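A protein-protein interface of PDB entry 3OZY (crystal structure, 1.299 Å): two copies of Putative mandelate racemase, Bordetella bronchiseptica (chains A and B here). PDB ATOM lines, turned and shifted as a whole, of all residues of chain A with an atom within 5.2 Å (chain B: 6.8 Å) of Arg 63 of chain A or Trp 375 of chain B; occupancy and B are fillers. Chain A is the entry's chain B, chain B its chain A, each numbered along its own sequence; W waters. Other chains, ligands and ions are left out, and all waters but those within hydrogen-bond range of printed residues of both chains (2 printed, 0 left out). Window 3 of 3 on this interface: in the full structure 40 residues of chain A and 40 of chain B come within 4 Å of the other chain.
The side-chain carboxylate (OD1) of Asp 57 of chain B lies within salt-bridge range of the guanidinium group (NH2) of Arg 63 of chain A (2.8 Å).
The side-chain carboxylate (OD2) of Asp 57 of chain B is in hydrogen-bond range of the backbone NH (N) of Ala 59 of chain B (3.0 Å).
NH1 of Arg 63 of chain A is in salt-bridge range of OD2 of Asp 67 of chain A.
O of Glu 378 of chain B sits at hydrogen-bond distance from NE1 of Trp 375 of chain B, at 2.9 Å.
OD2 of Asp 57 of chain B lies within hydrogen-bond range of N of Val 60 of chain B (3.0 Å).
The backbone carbonyl oxygen (O) of Ala 12 of chain B sits at hydrogen-bond distance from the backbone NH (N) of Trp 375 of chain B, 2.9 Å away.
The backbone carbonyl oxygen (O) of Arg 63 of chain A is in hydrogen-bond range of the backbone NH (N) of Val 68 of chain A.
Arg 63 of chain A touches Ala 59 of chain B (NE to CB, 3.5 Å).
Val 60 of chain B touches Arg 63 of chain A (CG2 to CG, 3.7 Å).
Arg 63 of chain A touches Trp 375 of chain B (NH2 to CH2, 3.5 Å).
Val 68 of chain A touches Asp 57 of chain B (CG2 to CB, 3.9 Å).
Arg 63 of chain A touches four residues of chain B.
Printed residues of chain B within 4 Å of Val 68 of chain A: Asp 57 (3.9 Å).
Of the printed residues of chain A, Asp 57 of chain B touches Arg 63 (2.8 Å) and Val 68 (3.9 Å).
Of the printed residues of chain A, Ala 59 of chain B touches Arg 63.
Of the printed residues of chain A, Val 60 of chain B touches Arg 63 (3.7 Å).
Trp 375 of chain B touches one residue of chain A.
The nearest residue of chain B that does not touch Arg 63 of chain A is Gly 377 of chain B (5.5 Å).
The nearest printed residue of chain A that does not touch Val 60 of chain B is Val 60 of chain A (4.1 Å).
Of the 11 printed residues of chain A, 2 touch a printed residue of chain B.
Hydrophobic or aromatic side chains of chain A that line the printed part of chain B: Val 68.
Hydrophobic or aromatic side chains of chain B that line the printed part of chain A: Ala 59, Val 60 and Trp 375.
Among the printed residues, 5 pairs touch across the chains.
Positions printed for both chains: 58, 59, 60 and 62.
Of the 5 pairs that touch across the chains among the printed residues, none has its exchanged pair printed and touching as well.
Water W1 lies within hydrogen-bond range of the backbone carbonyl oxygen of Gly 377 of chain B (2.9 Å) and the guanidinium group of Arg 63 of chain A (2.9 Å).
Water W2 bridges the backbone carbonyl oxygen of Ala 59 of chain A (3.2 Å) and the backbone carbonyl oxygen of Ala 59 of chain B (3.2 Å).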
ATOM      1  N   LEU A  58      12.108 -10.200  30.925  1.00  0.00           N
ATOM      2  CA  LEU A  58      13.304 -11.033  30.840  1.00  0.00           C
ATOM      3  C   LEU A  58      13.869 -11.165  29.427  1.00  0.00           C
ATOM      4  O   LEU A  58      15.085 -11.282  29.264  1.00  0.00           O
ATOM      5  CB  LEU A  58      13.057 -12.421  31.438  1.00  0.00           C
ATOM      6  CG  LEU A  58      12.724 -12.485  32.925  1.00  0.00           C
ATOM      7  CD1 LEU A  58      12.620 -13.938  33.348  1.00  0.00           C
ATOM      8  CD2 LEU A  58      13.778 -11.779  33.761  1.00  0.00           C
ATOM      9  N   ALA A  59      13.000 -11.148  28.419  1.00  0.00           N
ATOM     10  CA  ALA A  59      13.470 -11.238  27.037  1.00  0.00           C
ATOM     11  C   ALA A  59      14.184  -9.947  26.637  1.00  0.00           C
ATOM     12  O   ALA A  59      15.202  -9.979  25.938  1.00  0.00           O
ATOM     13  CB  ALA A  59      12.318 -11.529  26.092  1.00  0.00           C
ATOM     14  N   VAL A  60      13.661  -8.807  27.084  1.00  0.00           N
ATOM     15  CA  VAL A  60      14.327  -7.531  26.829  1.00  0.00           C
ATOM     16  C   VAL A  60      15.715  -7.546  27.461  1.00  0.00           C
ATOM     17  O   VAL A  60      16.710  -7.202  26.811  1.00  0.00           O
ATOM     18  CB  VAL A  60      13.499  -6.348  27.362  1.00  0.00           C
ATOM     19  CG1 VAL A  60      14.348  -5.076  27.380  1.00  0.00           C
ATOM     20  CG2 VAL A  60      12.251  -6.164  26.512  1.00  0.00           C
ATOM     21  N   LEU A  61      15.793  -7.966  28.720  1.00  0.00           N
ATOM     22  CA  LEU A  61      17.077  -8.040  29.408  1.00  0.00           C
ATOM     23  C   LEU A  61      18.051  -8.993  28.725  1.00  0.00           C
ATOM     24  O   LEU A  61      19.224  -8.662  28.525  1.00  0.00           O
ATOM     25  CB  LEU A  61      16.897  -8.443  30.868  1.00  0.00           C
ATOM     26  CG  LEU A  61      16.417  -7.367  31.842  1.00  0.00           C
ATOM     27  CD1 LEU A  61      16.071  -8.010  33.171  1.00  0.00           C
ATOM     28  CD2 LEU A  61      17.481  -6.283  32.020  1.00  0.00           C
ATOM     29  N   LYS A  62      17.571 -10.184  28.384  1.00  0.00           N
ATOM     30  CA  LYS A  62      18.427 -11.203  27.779  1.00  0.00           C
ATOM     31  C   LYS A  62      19.019 -10.703  26.463  1.00  0.00           C
ATOM     32  O   LYS A  62      20.225 -10.836  26.224  1.00  0.00           O
ATOM     33  CB  LYS A  62      17.647 -12.506  27.574  1.00  0.00           C
ATOM     34  CG  LYS A  62      18.455 -13.638  26.931  1.00  0.00           C
ATOM     35  CD  LYS A  62      17.590 -14.895  26.814  1.00  0.00           C
ATOM     36  CE  LYS A  62      18.341 -16.073  26.187  1.00  0.00           C
ATOM     37  NZ  LYS A  62      19.435 -16.575  27.057  1.00  0.00           N
ATOM     38  N   ARG A  63      18.177 -10.128  25.621  1.00  0.00           N
ATOM     39  CA  ARG A  63      18.634  -9.579  24.348  1.00  0.00           C
ATOM     40  C   ARG A  63      19.623  -8.435  24.564  1.00  0.00           C
ATOM     41  O   ARG A  63      20.678  -8.384  23.926  1.00  0.00           O
ATOM     42  CB  ARG A  63      17.431  -9.091  23.545  1.00  0.00           C
ATOM     43  CG  ARG A  63      17.777  -8.401  22.246  1.00  0.00           C
ATOM     44  CD  ARG A  63      18.260  -9.360  21.176  1.00  0.00           C
ATOM     45  NE  ARG A  63      18.759  -8.584  20.046  1.00  0.00           N
ATOM     46  CZ  ARG A  63      19.366  -9.091  18.978  1.00  0.00           C
ATOM     47  NH1 ARG A  63      19.548 -10.402  18.867  1.00  0.00           N
ATOM     48  NH2 ARG A  63      19.784  -8.276  18.019  1.00  0.00           N
ATOM     49  N   ALA A  64      19.304  -7.514  25.467  1.00  0.00           N
ATOM     50  CA  ALA A  64      20.211  -6.399  25.707  1.00  0.00           C
ATOM     51  C   ALA A  64      21.567  -6.890  26.181  1.00  0.00           C
ATOM     52  O   ALA A  64      22.605  -6.400  25.742  1.00  0.00           O
ATOM     53  CB  ALA A  64      19.621  -5.430  26.718  1.00  0.00           C
ATOM     54  N   ILE A  65      21.565  -7.864  27.079  1.00  0.00           N
ATOM     55  CA  ILE A  65      22.802  -8.358  27.644  1.00  0.00           C
ATOM     56  C   ILE A  65      23.622  -9.167  26.635  1.00  0.00           C
ATOM     57  O   ILE A  65      24.817  -8.922  26.465  1.00  0.00           O
ATOM     58  CB  ILE A  65      22.526  -9.160  28.932  1.00  0.00           C
ATOM     59  CG1 ILE A  65      22.013  -8.205  30.025  1.00  0.00           C
ATOM     60  CG2 ILE A  65      23.772  -9.902  29.400  1.00  0.00           C
ATOM     61  CD1 ILE A  65      21.383  -8.905  31.232  1.00  0.00           C
ATOM     62  N   GLU A  66      22.987 -10.128  25.965  1.00  0.00           N
ATOM     63  CA  GLU A  66      23.728 -11.026  25.072  1.00  0.00           C
ATOM     64  C   GLU A  66      24.102 -10.385  23.744  1.00  0.00           C
ATOM     65  O   GLU A  66      25.174 -10.658  23.202  1.00  0.00           O
ATOM     66  CB  GLU A  66      22.936 -12.315  24.827  1.00  0.00           C
ATOM     67  CG  GLU A  66      22.756 -13.136  26.104  1.00  0.00           C
ATOM     68  CD  GLU A  66      22.054 -14.466  25.889  1.00  0.00           C
ATOM     69  OE1 GLU A  66      21.531 -14.714  24.778  1.00  0.00           O
ATOM     70  OE2 GLU A  66      22.039 -15.272  26.844  1.00  0.00           O
ATOM     71  N   ASP A  67      23.234  -9.526  23.227  1.00  0.00           N
ATOM     72  CA  ASP A  67      23.357  -9.109  21.836  1.00  0.00           C
ATOM     73  C   ASP A  67      23.590  -7.616  21.618  1.00  0.00           C
ATOM     74  O   ASP A  67      23.890  -7.198  20.495  1.00  0.00           O
ATOM     75  CB  ASP A  67      22.124  -9.573  21.063  1.00  0.00           C
ATOM     76  CG  ASP A  67      21.930 -11.073  21.138  1.00  0.00           C
ATOM     77  OD1 ASP A  67      22.854 -11.805  20.736  1.00  0.00           O
ATOM     78  OD2 ASP A  67      20.867 -11.519  21.616  1.00  0.00           O
ATOM     79  N   VAL A  68      23.447  -6.808  22.666  1.00  0.00           N
ATOM     80  CA  VAL A  68      23.774  -5.391  22.561  1.00  0.00           C
ATOM     81  C   VAL A  68      25.049  -5.107  23.354  1.00  0.00           C
ATOM     82  O   VAL A  68      26.038  -4.609  22.811  1.00  0.00           O
ATOM     83  CB  VAL A  68      22.607  -4.486  23.030  1.00  0.00           C
ATOM     84  CG1 VAL A  68      23.006  -3.022  22.921  1.00  0.00           C
ATOM     85  CG2 VAL A  68      21.355  -4.753  22.197  1.00  0.00           C
ATOM     86  N   HIS B  11       6.822  -5.168  13.100  1.00  0.00           N
ATOM     87  CA  HIS B  11       7.567  -5.756  11.978  1.00  0.00           C
ATOM     88  C   HIS B  11       8.982  -5.206  11.949  1.00  0.00           C
ATOM     89  O   HIS B  11       9.183  -4.025  11.693  1.00  0.00           O
ATOM     90  CB  HIS B  11       6.905  -5.427  10.632  1.00  0.00           C
ATOM     91  CG  HIS B  11       5.461  -5.811  10.539  1.00  0.00           C
ATOM     92  ND1 HIS B  11       5.041  -7.020  10.023  1.00  0.00           N
ATOM     93  CD2 HIS B  11       4.338  -5.132  10.868  1.00  0.00           C
ATOM     94  CE1 HIS B  11       3.720  -7.074  10.059  1.00  0.00           C
ATOM     95  NE2 HIS B  11       3.270  -5.942  10.568  1.00  0.00           N
ATOM     96  N   ALA B  12       9.965  -6.063  12.192  1.00  0.00           N
ATOM     97  CA  ALA B  12      11.365  -5.651  12.134  1.00  0.00           C
ATOM     98  C   ALA B  12      11.875  -5.615  10.697  1.00  0.00           C
ATOM     99  O   ALA B  12      11.835  -6.629   9.989  1.00  0.00           O
ATOM    100  CB  ALA B  12      12.223  -6.568  12.985  1.00  0.00           C
ATOM    101  N   LEU B  13      12.370  -4.450  10.281  1.00  0.00           N
ATOM    102  CA  LEU B  13      12.809  -4.231   8.909  1.00  0.00           C
ATOM    103  C   LEU B  13      14.247  -3.733   8.842  1.00  0.00           C
ATOM    104  O   LEU B  13      14.686  -2.949   9.687  1.00  0.00           O
ATOM    105  CB  LEU B  13      11.900  -3.211   8.223  1.00  0.00           C
ATOM    106  CG  LEU B  13      10.400  -3.485   8.222  1.00  0.00           C
ATOM    107  CD1 LEU B  13       9.664  -2.380   7.472  1.00  0.00           C
ATOM    108  CD2 LEU B  13      10.110  -4.836   7.584  1.00  0.00           C
ATOM    109  N   SER B  14      14.982  -4.190   7.828  1.00  0.00           N
ATOM    110  CA  SER B  14      16.335  -3.709   7.603  1.00  0.00           C
ATOM    111  C   SER B  14      16.550  -3.409   6.127  1.00  0.00           C
ATOM    112  O   SER B  14      16.085  -4.153   5.257  1.00  0.00           O
ATOM    113  CB  SER B  14      17.366  -4.722   8.103  1.00  0.00           C
ATOM    114  OG  SER B  14      18.669  -4.154   8.102  1.00  0.00           O
ATOM    115  N   GLN B  34      17.293   0.802   9.632  1.00  0.00           N
ATOM    116  CA  GLN B  34      16.330  -0.148  10.164  1.00  0.00           C
ATOM    117  C   GLN B  34      15.161   0.563  10.823  1.00  0.00           C
ATOM    118  O   GLN B  34      15.223   1.761  11.119  1.00  0.00           O
ATOM    119  CB  GLN B  34      17.011  -1.057  11.192  1.00  0.00           C
ATOM    120  CG  GLN B  34      18.237  -1.776  10.630  1.00  0.00           C
ATOM    121  CD  GLN B  34      18.803  -2.837  11.560  1.00  0.00           C
ATOM    122  OE1 GLN B  34      18.694  -2.753  12.787  1.00  0.00           O
ATOM    123  NE2 GLN B  34      19.429  -3.845  10.972  1.00  0.00           N
ATOM    124  N   MET B  35      14.099  -0.198  11.067  1.00  0.00           N
ATOM    125  CA  MET B  35      12.956   0.309  11.815  1.00  0.00           C
ATOM    126  C   MET B  35      12.086  -0.844  12.257  1.00  0.00           C
ATOM    127  O   MET B  35      12.204  -1.972  11.760  1.00  0.00           O
ATOM    128  CB  MET B  35      12.102   1.241  10.950  1.00  0.00           C
ATOM    129  CG  MET B  35      11.341   0.518   9.838  1.00  0.00           C
ATOM    130  SD  MET B  35      10.352   1.611   8.799  1.00  0.00           S
ATOM    131  CE  MET B  35       9.086   2.102   9.970  1.00  0.00           C
ATOM    132  N   ILE B  36      11.225  -0.549  13.221  1.00  0.00           N
ATOM    133  CA  ILE B  36      10.041  -1.352  13.470  1.00  0.00           C
ATOM    134  C   ILE B  36       8.850  -0.643  12.847  1.00  0.00           C
ATOM    135  O   ILE B  36       8.626   0.541  13.095  1.00  0.00           O
ATOM    136  CB  ILE B  36       9.758  -1.479  14.979  1.00  0.00           C
ATOM    137  CG1 ILE B  36      10.783  -2.383  15.655  1.00  0.00           C
ATOM    138  CG2 ILE B  36       8.335  -1.992  15.217  1.00  0.00           C
ATOM    139  CD1 ILE B  36      10.654  -3.859  15.292  1.00  0.00           C
ATOM    140  N   ASP B  57      17.859  -1.485  19.198  1.00  0.00           N
ATOM    141  CA  ASP B  57      17.833  -2.895  18.807  1.00  0.00           C
ATOM    142  C   ASP B  57      16.425  -3.352  18.433  1.00  0.00           C
ATOM    143  O   ASP B  57      15.471  -3.142  19.185  1.00  0.00           O
ATOM    144  CB  ASP B  57      18.369  -3.774  19.929  1.00  0.00           C
ATOM    145  CG  ASP B  57      18.451  -5.223  19.520  1.00  0.00           C
ATOM    146  OD1 ASP B  57      19.450  -5.595  18.871  1.00  0.00           O
ATOM    147  OD2 ASP B  57      17.501  -5.983  19.821  1.00  0.00           O
ATOM    148  N   LEU B  58      16.296  -3.996  17.276  1.00  0.00           N
ATOM    149  CA  LEU B  58      14.976  -4.331  16.756  1.00  0.00           C
ATOM    150  C   LEU B  58      14.273  -5.406  17.580  1.00  0.00           C
ATOM    151  O   LEU B  58      13.051  -5.362  17.706  1.00  0.00           O
ATOM    152  CB  LEU B  58      15.037  -4.752  15.285  1.00  0.00           C
ATOM    153  CG  LEU B  58      15.482  -3.685  14.289  1.00  0.00           C
ATOM    154  CD1 LEU B  58      15.299  -4.224  12.869  1.00  0.00           C
ATOM    155  CD2 LEU B  58      14.709  -2.382  14.464  1.00  0.00           C
ATOM    156  N   ALA B  59      15.026  -6.363  18.121  1.00  0.00           N
ATOM    157  CA  ALA B  59      14.419  -7.403  18.957  1.00  0.00           C
ATOM    158  C   ALA B  59      13.924  -6.812  20.278  1.00  0.00           C
ATOM    159  O   ALA B  59      12.839  -7.164  20.751  1.00  0.00           O
ATOM    160  CB  ALA B  59      15.389  -8.542  19.200  1.00  0.00           C
ATOM    161  N   VAL B  60      14.706  -5.910  20.872  1.00  0.00           N
ATOM    162  CA  VAL B  60      14.255  -5.215  22.079  1.00  0.00           C
ATOM    163  C   VAL B  60      12.951  -4.462  21.808  1.00  0.00           C
ATOM    164  O   VAL B  60      11.984  -4.591  22.560  1.00  0.00           O
ATOM    165  CB  VAL B  60      15.330  -4.250  22.609  1.00  0.00           C
ATOM    166  CG1 VAL B  60      14.761  -3.340  23.694  1.00  0.00           C
ATOM    167  CG2 VAL B  60      16.521  -5.026  23.139  1.00  0.00           C
ATOM    168  N   LYS B  62      10.726  -4.950  19.346  1.00  0.00           N
ATOM    169  CA  LYS B  62       9.645  -5.872  19.016  1.00  0.00           C
ATOM    170  C   LYS B  62       9.045  -6.498  20.270  1.00  0.00           C
ATOM    171  O   LYS B  62       7.820  -6.565  20.422  1.00  0.00           O
ATOM    172  CB  LYS B  62      10.141  -6.955  18.057  1.00  0.00           C
ATOM    173  CG  LYS B  62       9.079  -7.972  17.662  1.00  0.00           C
ATOM    174  CD  LYS B  62       9.675  -8.982  16.678  1.00  0.00           C
ATOM    175  CE  LYS B  62       8.654 -10.004  16.192  1.00  0.00           C
ATOM    176  NZ  LYS B  62       7.615  -9.413  15.304  1.00  0.00           N
ATOM    177  N   VAL B 370       7.647  -4.120   2.582  1.00  0.00           N
ATOM    178  CA  VAL B 370       7.757  -4.597   3.958  1.00  0.00           C
ATOM    179  C   VAL B 370       8.116  -6.081   3.997  1.00  0.00           C
ATOM    180  O   VAL B 370       9.067  -6.487   4.661  1.00  0.00           O
ATOM    181  CB  VAL B 370       6.450  -4.345   4.745  1.00  0.00           C
ATOM    182  CG1 VAL B 370       6.499  -5.015   6.113  1.00  0.00           C
ATOM    183  CG2 VAL B 370       6.204  -2.842   4.884  1.00  0.00           C
ATOM    184  N   HIS B 373      11.774  -6.986   3.163  1.00  0.00           N
ATOM    185  CA  HIS B 373      12.873  -6.416   3.945  1.00  0.00           C
ATOM    186  C   HIS B 373      12.859  -6.810   5.417  1.00  0.00           C
ATOM    187  O   HIS B 373      13.282  -6.036   6.288  1.00  0.00           O
ATOM    188  CB  HIS B 373      12.932  -4.897   3.769  1.00  0.00           C
ATOM    189  CG  HIS B 373      13.317  -4.484   2.386  1.00  0.00           C
ATOM    190  ND1 HIS B 373      12.401  -4.378   1.362  1.00  0.00           N
ATOM    191  CD2 HIS B 373      14.523  -4.188   1.847  1.00  0.00           C
ATOM    192  CE1 HIS B 373      13.025  -4.020   0.253  1.00  0.00           C
ATOM    193  NE2 HIS B 373      14.312  -3.895   0.521  1.00  0.00           N
ATOM    194  N   ALA B 374      12.401  -8.021   5.695  1.00  0.00           N
ATOM    195  CA  ALA B 374      12.453  -8.537   7.055  1.00  0.00           C
ATOM    196  C   ALA B 374      13.885  -8.565   7.586  1.00  0.00           C
ATOM    197  O   ALA B 374      14.816  -8.997   6.906  1.00  0.00           O
ATOM    198  CB  ALA B 374      11.825  -9.922   7.128  1.00  0.00           C
ATOM    199  N   TRP B 375      14.053  -8.098   8.816  1.00  0.00           N
ATOM    200  CA  TRP B 375      15.334  -8.108   9.498  1.00  0.00           C
ATOM    201  C   TRP B 375      15.849  -9.531   9.674  1.00  0.00           C
ATOM    202  O   TRP B 375      15.086 -10.440  10.008  1.00  0.00           O
ATOM    203  CB  TRP B 375      15.145  -7.443  10.858  1.00  0.00           C
ATOM    204  CG  TRP B 375      16.332  -7.362  11.768  1.00  0.00           C
ATOM    205  CD1 TRP B 375      17.564  -6.833  11.498  1.00  0.00           C
ATOM    206  CD2 TRP B 375      16.353  -7.743  13.148  1.00  0.00           C
ATOM    207  NE1 TRP B 375      18.359  -6.891  12.621  1.00  0.00           N
ATOM    208  CE2 TRP B 375      17.637  -7.450  13.646  1.00  0.00           C
ATOM    209  CE3 TRP B 375      15.410  -8.326  14.006  1.00  0.00           C
ATOM    210  CZ2 TRP B 375      18.004  -7.712  14.969  1.00  0.00           C
ATOM    211  CZ3 TRP B 375      15.772  -8.585  15.315  1.00  0.00           C
ATOM    212  CH2 TRP B 375      17.056  -8.280  15.785  1.00  0.00           C
ATOM    213  N   LYS B 376      17.145  -9.717   9.445  1.00  0.00           N
ATOM    214  CA  LYS B 376      17.775 -11.025   9.618  1.00  0.00           C
ATOM    215  C   LYS B 376      18.949 -10.973  10.596  1.00  0.00           C
ATOM    216  O   LYS B 376      19.880 -11.775  10.515  1.00  0.00           O
ATOM    217  CB  LYS B 376      18.216 -11.601   8.266  1.00  0.00           C
ATOM    218  CG  LYS B 376      17.065 -11.849   7.305  1.00  0.00           C
ATOM    219  CD  LYS B 376      17.557 -12.410   5.980  1.00  0.00           C
ATOM    220  CE  LYS B 376      16.411 -12.547   4.988  1.00  0.00           C
ATOM    221  NZ  LYS B 376      15.257 -13.288   5.574  1.00  0.00           N
ATOM    222  N   GLY B 377      18.908 -10.018  11.518  1.00  0.00           N
ATOM    223  CA  GLY B 377      19.942  -9.892  12.532  1.00  0.00           C
ATOM    224  C   GLY B 377      21.055  -8.904  12.207  1.00  0.00           C
ATOM    225  O   GLY B 377      22.000  -8.772  12.981  1.00  0.00           O
ATOM    226  N   GLU B 378      20.950  -8.212  11.073  1.00  0.00           N
ATOM    227  CA  GLU B 378      21.933  -7.195  10.697  1.00  0.00           C
ATOM    228  C   GLU B 378      22.003  -6.090  11.755  1.00  0.00           C
ATOM    229  O   GLU B 378      20.994  -5.767  12.394  1.00  0.00           O
ATOM    230  CB  GLU B 378      21.571  -6.564   9.352  1.00  0.00           C
ATOM    231  CG  GLU B 378      21.461  -7.550   8.194  1.00  0.00           C
ATOM    232  CD  GLU B 378      20.032  -8.007   7.929  1.00  0.00           C
ATOM    233  OE1 GLU B 378      19.186  -7.957   8.851  1.00  0.00           O
ATOM    234  OE2 GLU B 378      19.755  -8.428   6.786  1.00  0.00           O
ATOM    235  N   PRO B 379      23.190  -5.503  11.945  1.00  0.00           N
ATOM    236  CA  PRO B 379      23.315  -4.363  12.859  1.00  0.00           C
ATOM    237  C   PRO B 379      22.879  -3.067  12.172  1.00  0.00           C
ATOM    238  O   PRO B 379      22.975  -2.960  10.948  1.00  0.00           O
ATOM    239  CB  PRO B 379      24.814  -4.328  13.139  1.00  0.00           C
ATOM    240  CG  PRO B 379      25.418  -4.784  11.839  1.00  0.00           C
ATOM    241  CD  PRO B 379      24.489  -5.874  11.349  1.00  0.00           C
ATOM    242  N   ALA B 380      22.409  -2.087  12.937  1.00  0.00           N
ATOM    243  CA  ALA B 380      22.032  -0.802  12.349  1.00  0.00           C
ATOM    244  C   ALA B 380      23.197   0.184  12.290  1.00  0.00           C
ATOM    245  O   ALA B 380      23.328   0.949  11.332  1.00  0.00           O
ATOM    246  CB  ALA B 380      20.863  -0.170  13.120  1.00  0.00           C
HETATM  247  O   HOH W   1      21.787  -8.229  15.857  1.00  0.00           O
HETATM  248  O   HOH W   2      14.009  -8.510  23.388  1.00  0.00           O
